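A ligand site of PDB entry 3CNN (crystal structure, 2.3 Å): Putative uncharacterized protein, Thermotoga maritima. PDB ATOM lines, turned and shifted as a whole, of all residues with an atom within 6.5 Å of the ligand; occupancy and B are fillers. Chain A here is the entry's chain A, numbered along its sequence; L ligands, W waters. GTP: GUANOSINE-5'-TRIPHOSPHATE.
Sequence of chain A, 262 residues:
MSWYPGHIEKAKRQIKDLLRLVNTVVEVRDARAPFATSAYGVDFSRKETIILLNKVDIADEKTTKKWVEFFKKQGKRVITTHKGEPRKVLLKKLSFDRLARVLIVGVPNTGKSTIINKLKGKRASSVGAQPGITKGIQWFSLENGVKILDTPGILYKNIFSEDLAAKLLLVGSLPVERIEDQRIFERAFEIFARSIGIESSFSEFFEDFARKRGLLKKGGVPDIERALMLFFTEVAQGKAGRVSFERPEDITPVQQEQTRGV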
ATOM      1  N   VAL A  28       8.235  35.809  14.169  1.00  0.00           N
ATOM      2  CA  VAL A  28       7.400  34.718  14.636  1.00  0.00           C
ATOM      3  C   VAL A  28       7.119  34.844  16.145  1.00  0.00           C
ATOM      4  O   VAL A  28       8.025  34.639  16.996  1.00  0.00           O
ATOM      5  CB  VAL A  28       8.062  33.375  14.339  1.00  0.00           C
ATOM      6  CG1 VAL A  28       7.164  32.218  14.793  1.00  0.00           C
ATOM      7  CG2 VAL A  28       8.443  33.257  12.845  1.00  0.00           C
ATOM      8  N   ASN A  54       1.879  32.935  15.635  1.00  0.00           N
ATOM      9  CA  ASN A  54       1.946  31.499  15.493  1.00  0.00           C
ATOM     10  C   ASN A  54       1.155  30.753  16.593  1.00  0.00           C
ATOM     11  O   ASN A  54       0.792  31.337  17.604  1.00  0.00           O
ATOM     12  CB  ASN A  54       3.415  31.072  15.470  1.00  0.00           C
ATOM     13  CG  ASN A  54       3.618  29.759  14.775  1.00  0.00           C
ATOM     14  OD1 ASN A  54       2.876  29.422  13.885  1.00  0.00           O
ATOM     15  ND2 ASN A  54       4.635  29.022  15.173  1.00  0.00           N
ATOM     16  N   LYS A  55       0.878  29.474  16.343  1.00  0.00           N
ATOM     17  CA  LYS A  55       0.279  28.555  17.301  1.00  0.00           C
ATOM     18  C   LYS A  55      -1.159  28.926  17.661  1.00  0.00           C
ATOM     19  O   LYS A  55      -1.541  28.818  18.836  1.00  0.00           O
ATOM     20  CB  LYS A  55       1.142  28.452  18.582  1.00  0.00           C
ATOM     21  CG  LYS A  55       2.570  28.014  18.363  1.00  0.00           C
ATOM     22  CD  LYS A  55       3.261  27.732  19.711  1.00  0.00           C
ATOM     23  CE  LYS A  55       4.661  27.185  19.535  1.00  0.00           C
ATOM     24  NZ  LYS A  55       5.436  27.149  20.813  1.00  0.00           N
ATOM     25  N   VAL A  56      -1.938  29.374  16.680  1.00  0.00           N
ATOM     26  CA  VAL A  56      -3.307  29.846  16.968  1.00  0.00           C
ATOM     27  C   VAL A  56      -4.184  28.657  17.327  1.00  0.00           C
ATOM     28  O   VAL A  56      -5.288  28.825  17.890  1.00  0.00           O
ATOM     29  CB  VAL A  56      -3.957  30.685  15.809  1.00  0.00           C
ATOM     30  CG1 VAL A  56      -3.149  31.946  15.540  1.00  0.00           C
ATOM     31  CG2 VAL A  56      -4.146  29.866  14.540  1.00  0.00           C
ATOM     32  N   ASP A  57      -3.654  27.462  17.047  1.00  0.00           N
ATOM     33  CA  ASP A  57      -4.362  26.213  17.302  1.00  0.00           C
ATOM     34  C   ASP A  57      -4.506  25.928  18.792  1.00  0.00           C
ATOM     35  O   ASP A  57      -5.458  25.269  19.221  1.00  0.00           O
ATOM     36  CB  ASP A  57      -3.694  25.041  16.555  1.00  0.00           C
ATOM     37  CG  ASP A  57      -2.247  24.850  16.943  1.00  0.00           C
ATOM     38  OD1 ASP A  57      -1.529  25.867  17.027  1.00  0.00           O
ATOM     39  OD2 ASP A  57      -1.802  23.698  17.173  1.00  0.00           O
ATOM     40  N   ILE A  58      -3.559  26.442  19.585  1.00  0.00           N
ATOM     41  CA  ILE A  58      -3.577  26.253  21.034  1.00  0.00           C
ATOM     42  C   ILE A  58      -3.835  27.565  21.787  1.00  0.00           C
ATOM     43  O   ILE A  58      -3.629  27.637  23.001  1.00  0.00           O
ATOM     44  CB  ILE A  58      -2.296  25.537  21.546  1.00  0.00           C
ATOM     45  CG1 ILE A  58      -1.028  26.347  21.182  1.00  0.00           C
ATOM     46  CG2 ILE A  58      -2.237  24.107  21.000  1.00  0.00           C
ATOM     47  CD1 ILE A  58       0.235  25.827  21.784  1.00  0.00           C
ATOM     48  N   THR A  81      -1.191  31.900  11.927  1.00  0.00           N
ATOM     49  CA  THR A  81      -1.012  30.555  11.359  1.00  0.00           C
ATOM     50  C   THR A  81      -0.666  29.546  12.449  1.00  0.00           C
ATOM     51  O   THR A  81      -0.606  29.906  13.611  1.00  0.00           O
ATOM     52  CB  THR A  81       0.064  30.549  10.252  1.00  0.00           C
ATOM     53  OG1 THR A  81       0.146  29.263   9.618  1.00  0.00           O
ATOM     54  CG2 THR A  81       1.432  30.932  10.808  1.00  0.00           C
ATOM     55  N   HIS A  82      -0.443  28.297  12.059  1.00  0.00           N
ATOM     56  CA  HIS A  82      -0.013  27.214  12.948  1.00  0.00           C
ATOM     57  C   HIS A  82       0.568  26.060  12.130  1.00  0.00           C
ATOM     58  O   HIS A  82       0.348  25.981  10.935  1.00  0.00           O
ATOM     59  CB  HIS A  82      -1.176  26.744  13.835  1.00  0.00           C
ATOM     60  CG  HIS A  82      -2.312  26.127  13.069  1.00  0.00           C
ATOM     61  ND1 HIS A  82      -2.451  24.755  12.940  1.00  0.00           N
ATOM     62  CD2 HIS A  82      -3.351  26.675  12.408  1.00  0.00           C
ATOM     63  CE1 HIS A  82      -3.523  24.494  12.212  1.00  0.00           C
ATOM     64  NE2 HIS A  82      -4.091  25.644  11.885  1.00  0.00           N
ATOM     65  N   LYS A  83       1.330  25.184  12.780  1.00  0.00           N
ATOM     66  CA  LYS A  83       1.852  23.924  12.227  1.00  0.00           C
ATOM     67  C   LYS A  83       0.979  23.289  11.133  1.00  0.00           C
ATOM     68  O   LYS A  83       1.448  23.050  10.019  1.00  0.00           O
ATOM     69  CB  LYS A  83       1.976  22.892  13.346  1.00  0.00           C
ATOM     70  CG  LYS A  83       3.343  22.705  13.913  1.00  0.00           C
ATOM     71  CD  LYS A  83       3.562  21.283  14.438  1.00  0.00           C
ATOM     72  CE  LYS A  83       2.783  20.969  15.728  1.00  0.00           C
ATOM     73  NZ  LYS A  83       1.330  20.587  15.524  1.00  0.00           N
ATOM     74  N   GLY A  84      -0.282  23.001  11.468  1.00  0.00           N
ATOM     75  CA  GLY A  84      -1.183  22.260  10.600  1.00  0.00           C
ATOM     76  C   GLY A  84      -1.630  22.961   9.326  1.00  0.00           C
ATOM     77  O   GLY A  84      -2.170  22.340   8.409  1.00  0.00           O
ATOM     78  N   GLY A 106      12.754  35.534  15.911  1.00  0.00           N
ATOM     79  CA  GLY A 106      11.927  35.479  17.108  1.00  0.00           C
ATOM     80  C   GLY A 106      12.661  34.989  18.344  1.00  0.00           C
ATOM     81  O   GLY A 106      13.772  34.436  18.258  1.00  0.00           O
ATOM     82  N   VAL A 107      12.022  35.195  19.498  1.00  0.00           N
ATOM     83  CA  VAL A 107      12.515  34.668  20.770  1.00  0.00           C
ATOM     84  C   VAL A 107      12.443  33.146  20.722  1.00  0.00           C
ATOM     85  O   VAL A 107      11.787  32.603  19.833  1.00  0.00           O
ATOM     86  CB  VAL A 107      11.785  35.320  21.990  1.00  0.00           C
ATOM     87  CG1 VAL A 107      11.892  36.853  21.920  1.00  0.00           C
ATOM     88  CG2 VAL A 107      10.318  34.866  22.099  1.00  0.00           C
ATOM     89  N   PRO A 108      13.168  32.440  21.610  1.00  0.00           N
ATOM     90  CA  PRO A 108      13.156  30.984  21.523  1.00  0.00           C
ATOM     91  C   PRO A 108      11.750  30.364  21.557  1.00  0.00           C
ATOM     92  O   PRO A 108      10.833  30.920  22.158  1.00  0.00           O
ATOM     93  CB  PRO A 108      13.935  30.548  22.769  1.00  0.00           C
ATOM     94  CG  PRO A 108      14.865  31.707  23.056  1.00  0.00           C
ATOM     95  CD  PRO A 108      14.043  32.922  22.699  1.00  0.00           C
ATOM     96  N   ASN A 109      11.619  29.213  20.896  1.00  0.00           N
ATOM     97  CA  ASN A 109      10.474  28.301  21.015  1.00  0.00           C
ATOM     98  C   ASN A 109       9.194  28.670  20.257  1.00  0.00           C
ATOM     99  O   ASN A 109       8.230  27.914  20.275  1.00  0.00           O
ATOM    100  CB  ASN A 109      10.157  28.038  22.502  1.00  0.00           C
ATOM    101  CG  ASN A 109       9.332  26.774  22.709  1.00  0.00           C
ATOM    102  OD1 ASN A 109       9.698  25.712  22.242  1.00  0.00           O
ATOM    103  ND2 ASN A 109       8.205  26.911  23.389  1.00  0.00           N
ATOM    104  N   THR A 110       9.176  29.818  19.585  1.00  0.00           N
ATOM    105  CA  THR A 110       7.935  30.319  18.950  1.00  0.00           C
ATOM    106  C   THR A 110       7.511  29.576  17.663  1.00  0.00           C
ATOM    107  O   THR A 110       6.416  29.805  17.123  1.00  0.00           O
ATOM    108  CB  THR A 110       7.986  31.831  18.733  1.00  0.00           C
ATOM    109  OG1 THR A 110       9.065  32.142  17.828  1.00  0.00           O
ATOM    110  CG2 THR A 110       8.220  32.523  20.085  1.00  0.00           C
ATOM    111  N   GLY A 111       8.378  28.671  17.199  1.00  0.00           N
ATOM    112  CA  GLY A 111       8.060  27.797  16.078  1.00  0.00           C
ATOM    113  C   GLY A 111       8.780  28.169  14.795  1.00  0.00           C
ATOM    114  O   GLY A 111       8.269  27.907  13.692  1.00  0.00           O
ATOM    115  N   LYS A 112       9.973  28.746  14.929  1.00  0.00           N
ATOM    116  CA  LYS A 112      10.729  29.282  13.794  1.00  0.00           C
ATOM    117  C   LYS A 112      11.277  28.220  12.848  1.00  0.00           C
ATOM    118  O   LYS A 112      11.225  28.387  11.626  1.00  0.00           O
ATOM    119  CB  LYS A 112      11.874  30.156  14.287  1.00  0.00           C
ATOM    120  CG  LYS A 112      11.434  31.375  15.059  1.00  0.00           C
ATOM    121  CD  LYS A 112      12.641  32.154  15.600  1.00  0.00           C
ATOM    122  CE  LYS A 112      13.492  31.356  16.580  1.00  0.00           C
ATOM    123  NZ  LYS A 112      12.738  31.049  17.811  1.00  0.00           N
ATOM    124  N   SER A 113      11.799  27.126  13.415  1.00  0.00           N
ATOM    125  CA  SER A 113      12.289  25.972  12.644  1.00  0.00           C
ATOM    126  C   SER A 113      11.150  25.267  11.915  1.00  0.00           C
ATOM    127  O   SER A 113      11.282  24.935  10.743  1.00  0.00           O
ATOM    128  CB  SER A 113      12.987  24.982  13.557  1.00  0.00           C
ATOM    129  OG  SER A 113      14.065  25.633  14.195  1.00  0.00           O
ATOM    130  N   THR A 114      10.052  25.039  12.619  1.00  0.00           N
ATOM    131  CA  THR A 114       8.849  24.429  12.044  1.00  0.00           C
ATOM    132  C   THR A 114       8.406  25.192  10.800  1.00  0.00           C
ATOM    133  O   THR A 114       8.107  24.576   9.771  1.00  0.00           O
ATOM    134  CB  THR A 114       7.712  24.378  13.078  1.00  0.00           C
ATOM    135  OG1 THR A 114       8.169  23.647  14.226  1.00  0.00           O
ATOM    136  CG2 THR A 114       6.458  23.680  12.508  1.00  0.00           C
ATOM    137  N   ILE A 115       8.385  26.516  10.885  1.00  0.00           N
ATOM    138  CA  ILE A 115       7.981  27.352   9.766  1.00  0.00           C
ATOM    139  C   ILE A 115       8.960  27.288   8.586  1.00  0.00           C
ATOM    140  O   ILE A 115       8.549  27.138   7.444  1.00  0.00           O
ATOM    141  CB  ILE A 115       7.651  28.788  10.202  1.00  0.00           C
ATOM    142  CG1 ILE A 115       6.284  28.792  10.922  1.00  0.00           C
ATOM    143  CG2 ILE A 115       7.648  29.737   9.013  1.00  0.00           C
ATOM    144  CD1 ILE A 115       6.036  29.990  11.820  1.00  0.00           C
ATOM    145  N   PRO A 152      16.981  30.568  11.377  1.00  0.00           N
ATOM    146  CA  PRO A 152      16.365  31.745  11.985  1.00  0.00           C
ATOM    147  C   PRO A 152      17.302  32.460  12.941  1.00  0.00           C
ATOM    148  O   PRO A 152      18.190  31.840  13.525  1.00  0.00           O
ATOM    149  CB  PRO A 152      15.174  31.160  12.751  1.00  0.00           C
ATOM    150  CG  PRO A 152      15.530  29.757  13.031  1.00  0.00           C
ATOM    151  CD  PRO A 152      16.612  29.317  12.079  1.00  0.00           C
ATOM    152  N   ILE A 154      17.690  33.921  16.496  1.00  0.00           N
ATOM    153  CA  ILE A 154      17.085  33.757  17.816  1.00  0.00           C
ATOM    154  C   ILE A 154      17.355  35.010  18.630  1.00  0.00           C
ATOM    155  O   ILE A 154      18.514  35.367  18.849  1.00  0.00           O
ATOM    156  CB  ILE A 154      17.599  32.499  18.539  1.00  0.00           C
ATOM    157  CG1 ILE A 154      17.291  31.264  17.686  1.00  0.00           C
ATOM    158  CG2 ILE A 154      16.959  32.368  19.923  1.00  0.00           C
ATOM    159  CD1 ILE A 154      18.120  30.007  17.995  1.00  0.00           C
ATOM    160  N   ALA A 236       3.072  25.302  27.720  1.00  0.00           N
ATOM    161  CA  ALA A 236       3.730  25.814  26.528  1.00  0.00           C
ATOM    162  C   ALA A 236       3.311  24.996  25.311  1.00  0.00           C
ATOM    163  O   ALA A 236       2.951  25.566  24.273  1.00  0.00           O
ATOM    164  CB  ALA A 236       5.249  25.785  26.690  1.00  0.00           C
ATOM    165  N   GLN A 237       3.326  23.677  25.490  1.00  0.00           N
ATOM    166  CA  GLN A 237       2.907  22.701  24.491  1.00  0.00           C
ATOM    167  C   GLN A 237       1.402  22.708  24.205  1.00  0.00           C
ATOM    168  O   GLN A 237       0.935  21.947  23.359  1.00  0.00           O
ATOM    169  CB  GLN A 237       3.349  21.291  24.914  1.00  0.00           C
ATOM    170  CG  GLN A 237       4.888  21.087  24.999  1.00  0.00           C
ATOM    171  CD  GLN A 237       5.306  19.686  25.524  1.00  0.00           C
ATOM    172  OE1 GLN A 237       4.459  18.874  25.923  1.00  0.00           O
ATOM    173  NE2 GLN A 237       6.613  19.415  25.509  1.00  0.00           N
ATOM    174  N   GLY A 238       0.642  23.556  24.887  1.00  0.00           N
ATOM    175  CA  GLY A 238      -0.805  23.635  24.665  1.00  0.00           C
ATOM    176  C   GLY A 238      -1.608  22.456  25.180  1.00  0.00           C
ATOM    177  O   GLY A 238      -2.766  22.274  24.775  1.00  0.00           O
HETATM  178  PG  GTP L   1      14.099  27.459  19.162  1.00  0.00           P
HETATM  179  O1G GTP L   1      14.391  28.933  18.866  1.00  0.00           O
HETATM  180  O2G GTP L   1      14.282  27.212  20.649  1.00  0.00           O
HETATM  181  O3G GTP L   1      15.059  26.521  18.432  1.00  0.00           O
HETATM  182  O3B GTP L   1      12.605  27.009  18.743  1.00  0.00           O
HETATM  183  PB  GTP L   1      11.893  27.395  17.350  1.00  0.00           P
HETATM  184  O1B GTP L   1      11.536  28.866  17.354  1.00  0.00           O
HETATM  185  O2B GTP L   1      12.754  27.036  16.170  1.00  0.00           O
HETATM  186  O3A GTP L   1      10.545  26.572  17.465  1.00  0.00           O
HETATM  187  PA  GTP L   1      10.227  25.065  17.045  1.00  0.00           P
HETATM  188  O1A GTP L   1       9.681  25.066  15.648  1.00  0.00           O
HETATM  189  O2A GTP L   1      11.331  24.079  17.286  1.00  0.00           O
HETATM  190  O5' GTP L   1       8.965  24.793  18.020  1.00  0.00           O
HETATM  191  C5' GTP L   1       9.106  24.487  19.385  1.00  0.00           C
HETATM  192  C4' GTP L   1       7.939  23.591  19.760  1.00  0.00           C
HETATM  193  O4' GTP L   1       6.736  24.193  19.354  1.00  0.00           O
HETATM  194  C3' GTP L   1       8.009  22.255  19.046  1.00  0.00           C
HETATM  195  O3' GTP L   1       7.646  21.247  19.959  1.00  0.00           O
HETATM  196  C2' GTP L   1       6.977  22.369  17.943  1.00  0.00           C
HETATM  197  O2' GTP L   1       6.419  21.109  17.685  1.00  0.00           O
HETATM  198  C1' GTP L   1       5.963  23.328  18.543  1.00  0.00           C
HETATM  199  N9  GTP L   1       5.189  24.138  17.568  1.00  0.00           N
HETATM  200  C8  GTP L   1       5.676  24.914  16.542  1.00  0.00           C
HETATM  201  N7  GTP L   1       4.624  25.497  15.927  1.00  0.00           N
HETATM  202  C5  GTP L   1       3.479  25.102  16.532  1.00  0.00           C
HETATM  203  C6  GTP L   1       2.126  25.397  16.306  1.00  0.00           C
HETATM  204  O6  GTP L   1       1.800  26.149  15.389  1.00  0.00           O
HETATM  205  N1  GTP L   1       1.158  24.832  17.124  1.00  0.00           N
HETATM  206  C2  GTP L   1       1.528  23.986  18.150  1.00  0.00           C
HETATM  207  N2  GTP L   1       0.612  23.432  18.931  1.00  0.00           N
HETATM  208  N3  GTP L   1       2.865  23.703  18.367  1.00  0.00           N
HETATM  209  C4  GTP L   1       3.820  24.247  17.575  1.00  0.00           C
HETATM  210  O   HOH W   1       3.512  22.848  21.082  1.00  0.00           O
HETATM  211  O   HOH W   2      15.306  28.272  16.072  1.00  0.00           O
HETATM  212  O   HOH W   3      14.351  24.165  17.399  1.00  0.00           O
HETATM  213  O   HOH W   4       5.516  26.817  13.654  1.00  0.00           O
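Water W4 lies within hydrogen-bond range of N7 of the ligand (2.8 Å), ND2 of Asn 54 (2.8 Å) and O of Gly 111 (3.0 Å).
Water W2 bridges an oxygen (O2B) of the ligand (2.8 Å) and the side-chain hydroxyl (OG) of Ser 113 (3.5 Å).
Asn 54 touches the ligand.
Lys 55 touches the ligand.
CG2 of Ile 58 touches N2 of the ligand (3.6 Å).
His 82 touches the ligand (CA to O6, 3.2 Å).
CA of Pro 108 touches O1G of the ligand (3.6 Å).
Ile 154 touches the ligand.
Hydrophobic or aromatic side chains within 4 Å of the ligand: Ile 58, His 82, Pro 108 and Ile 154.
14 residues have an atom within 4 Å of the ligand: Asn 54, Lys 55, Asp 57, Ile 58, His 82, Lys 83, Pro 108, Asn 109, Thr 110, Gly 111, Lys 112, Ser 113, Thr 114 and Ile 154.
The backbone NH (N) of Thr 114 is in hydrogen-bond range of an oxygen (O1A) of the ligand.
OG1 of Thr 114 sits at hydrogen-bond distance from O1A of the ligand (2.5 Å).
N of Lys 112 sits at hydrogen-bond distance from O1B of the ligand.
The side-chain amino group (NZ) of Lys 112 lies within salt-bridge range of an oxygen (O1B) of the ligand (2.5 Å).
The backbone NH of Ser 113 is in hydrogen-bond range of an oxygen (O2B) of the ligand, 2.9 Å away.
An oxygen (O2B) of the ligand is in hydrogen-bond range of the side-chain hydroxyl (OG) of Ser 113 (2.8 Å).
The backbone NH of Lys 83 lies within hydrogen-bond range of an oxygen (O6) of the ligand.
A nitrogen (N1) of the ligand lies within hydrogen-bond range of the side-chain carboxylate (OD1) of Asp 57.
An oxygen (O3A) of the ligand is in hydrogen-bond range of the backbone NH (N) of Gly 111, 3.0 Å away.
The backbone NH (N) of Asn 109 lies within hydrogen-bond range of an oxygen (O3B) of the ligand (3.2 Å).
The backbone NH (N) of Thr 110 is in hydrogen-bond range of an oxygen (O1B) of the ligand.
The side-chain amino group of Lys 112 is in hydrogen-bond range of the backbone carbonyl oxygen of Val 107, at 2.7 Å.
NZ of Lys 55 sits at hydrogen-bond distance from O of Asn 109, at 2.9 Å.
A ring nitrogen (ND1) of His 82 is in hydrogen-bond range of the backbone NH (N) of Gly 84 (3.2 Å).
The backbone NH (N) of Lys 55 sits at hydrogen-bond distance from the backbone carbonyl oxygen (O) of Thr 81, at 3.1 Å.
The side-chain amide nitrogen (ND2) of Asn 54 lies within hydrogen-bond range of the backbone carbonyl oxygen (O) of Thr 110 (2.8 Å).
The backbone carbonyl oxygen (O) of Val 107 lies within hydrogen-bond range of the side-chain hydroxyl (OG1) of Thr 110 (3.4 Å).
The side-chain hydroxyl of Thr 110 lies within hydrogen-bond range of the backbone carbonyl oxygen of Val 28.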
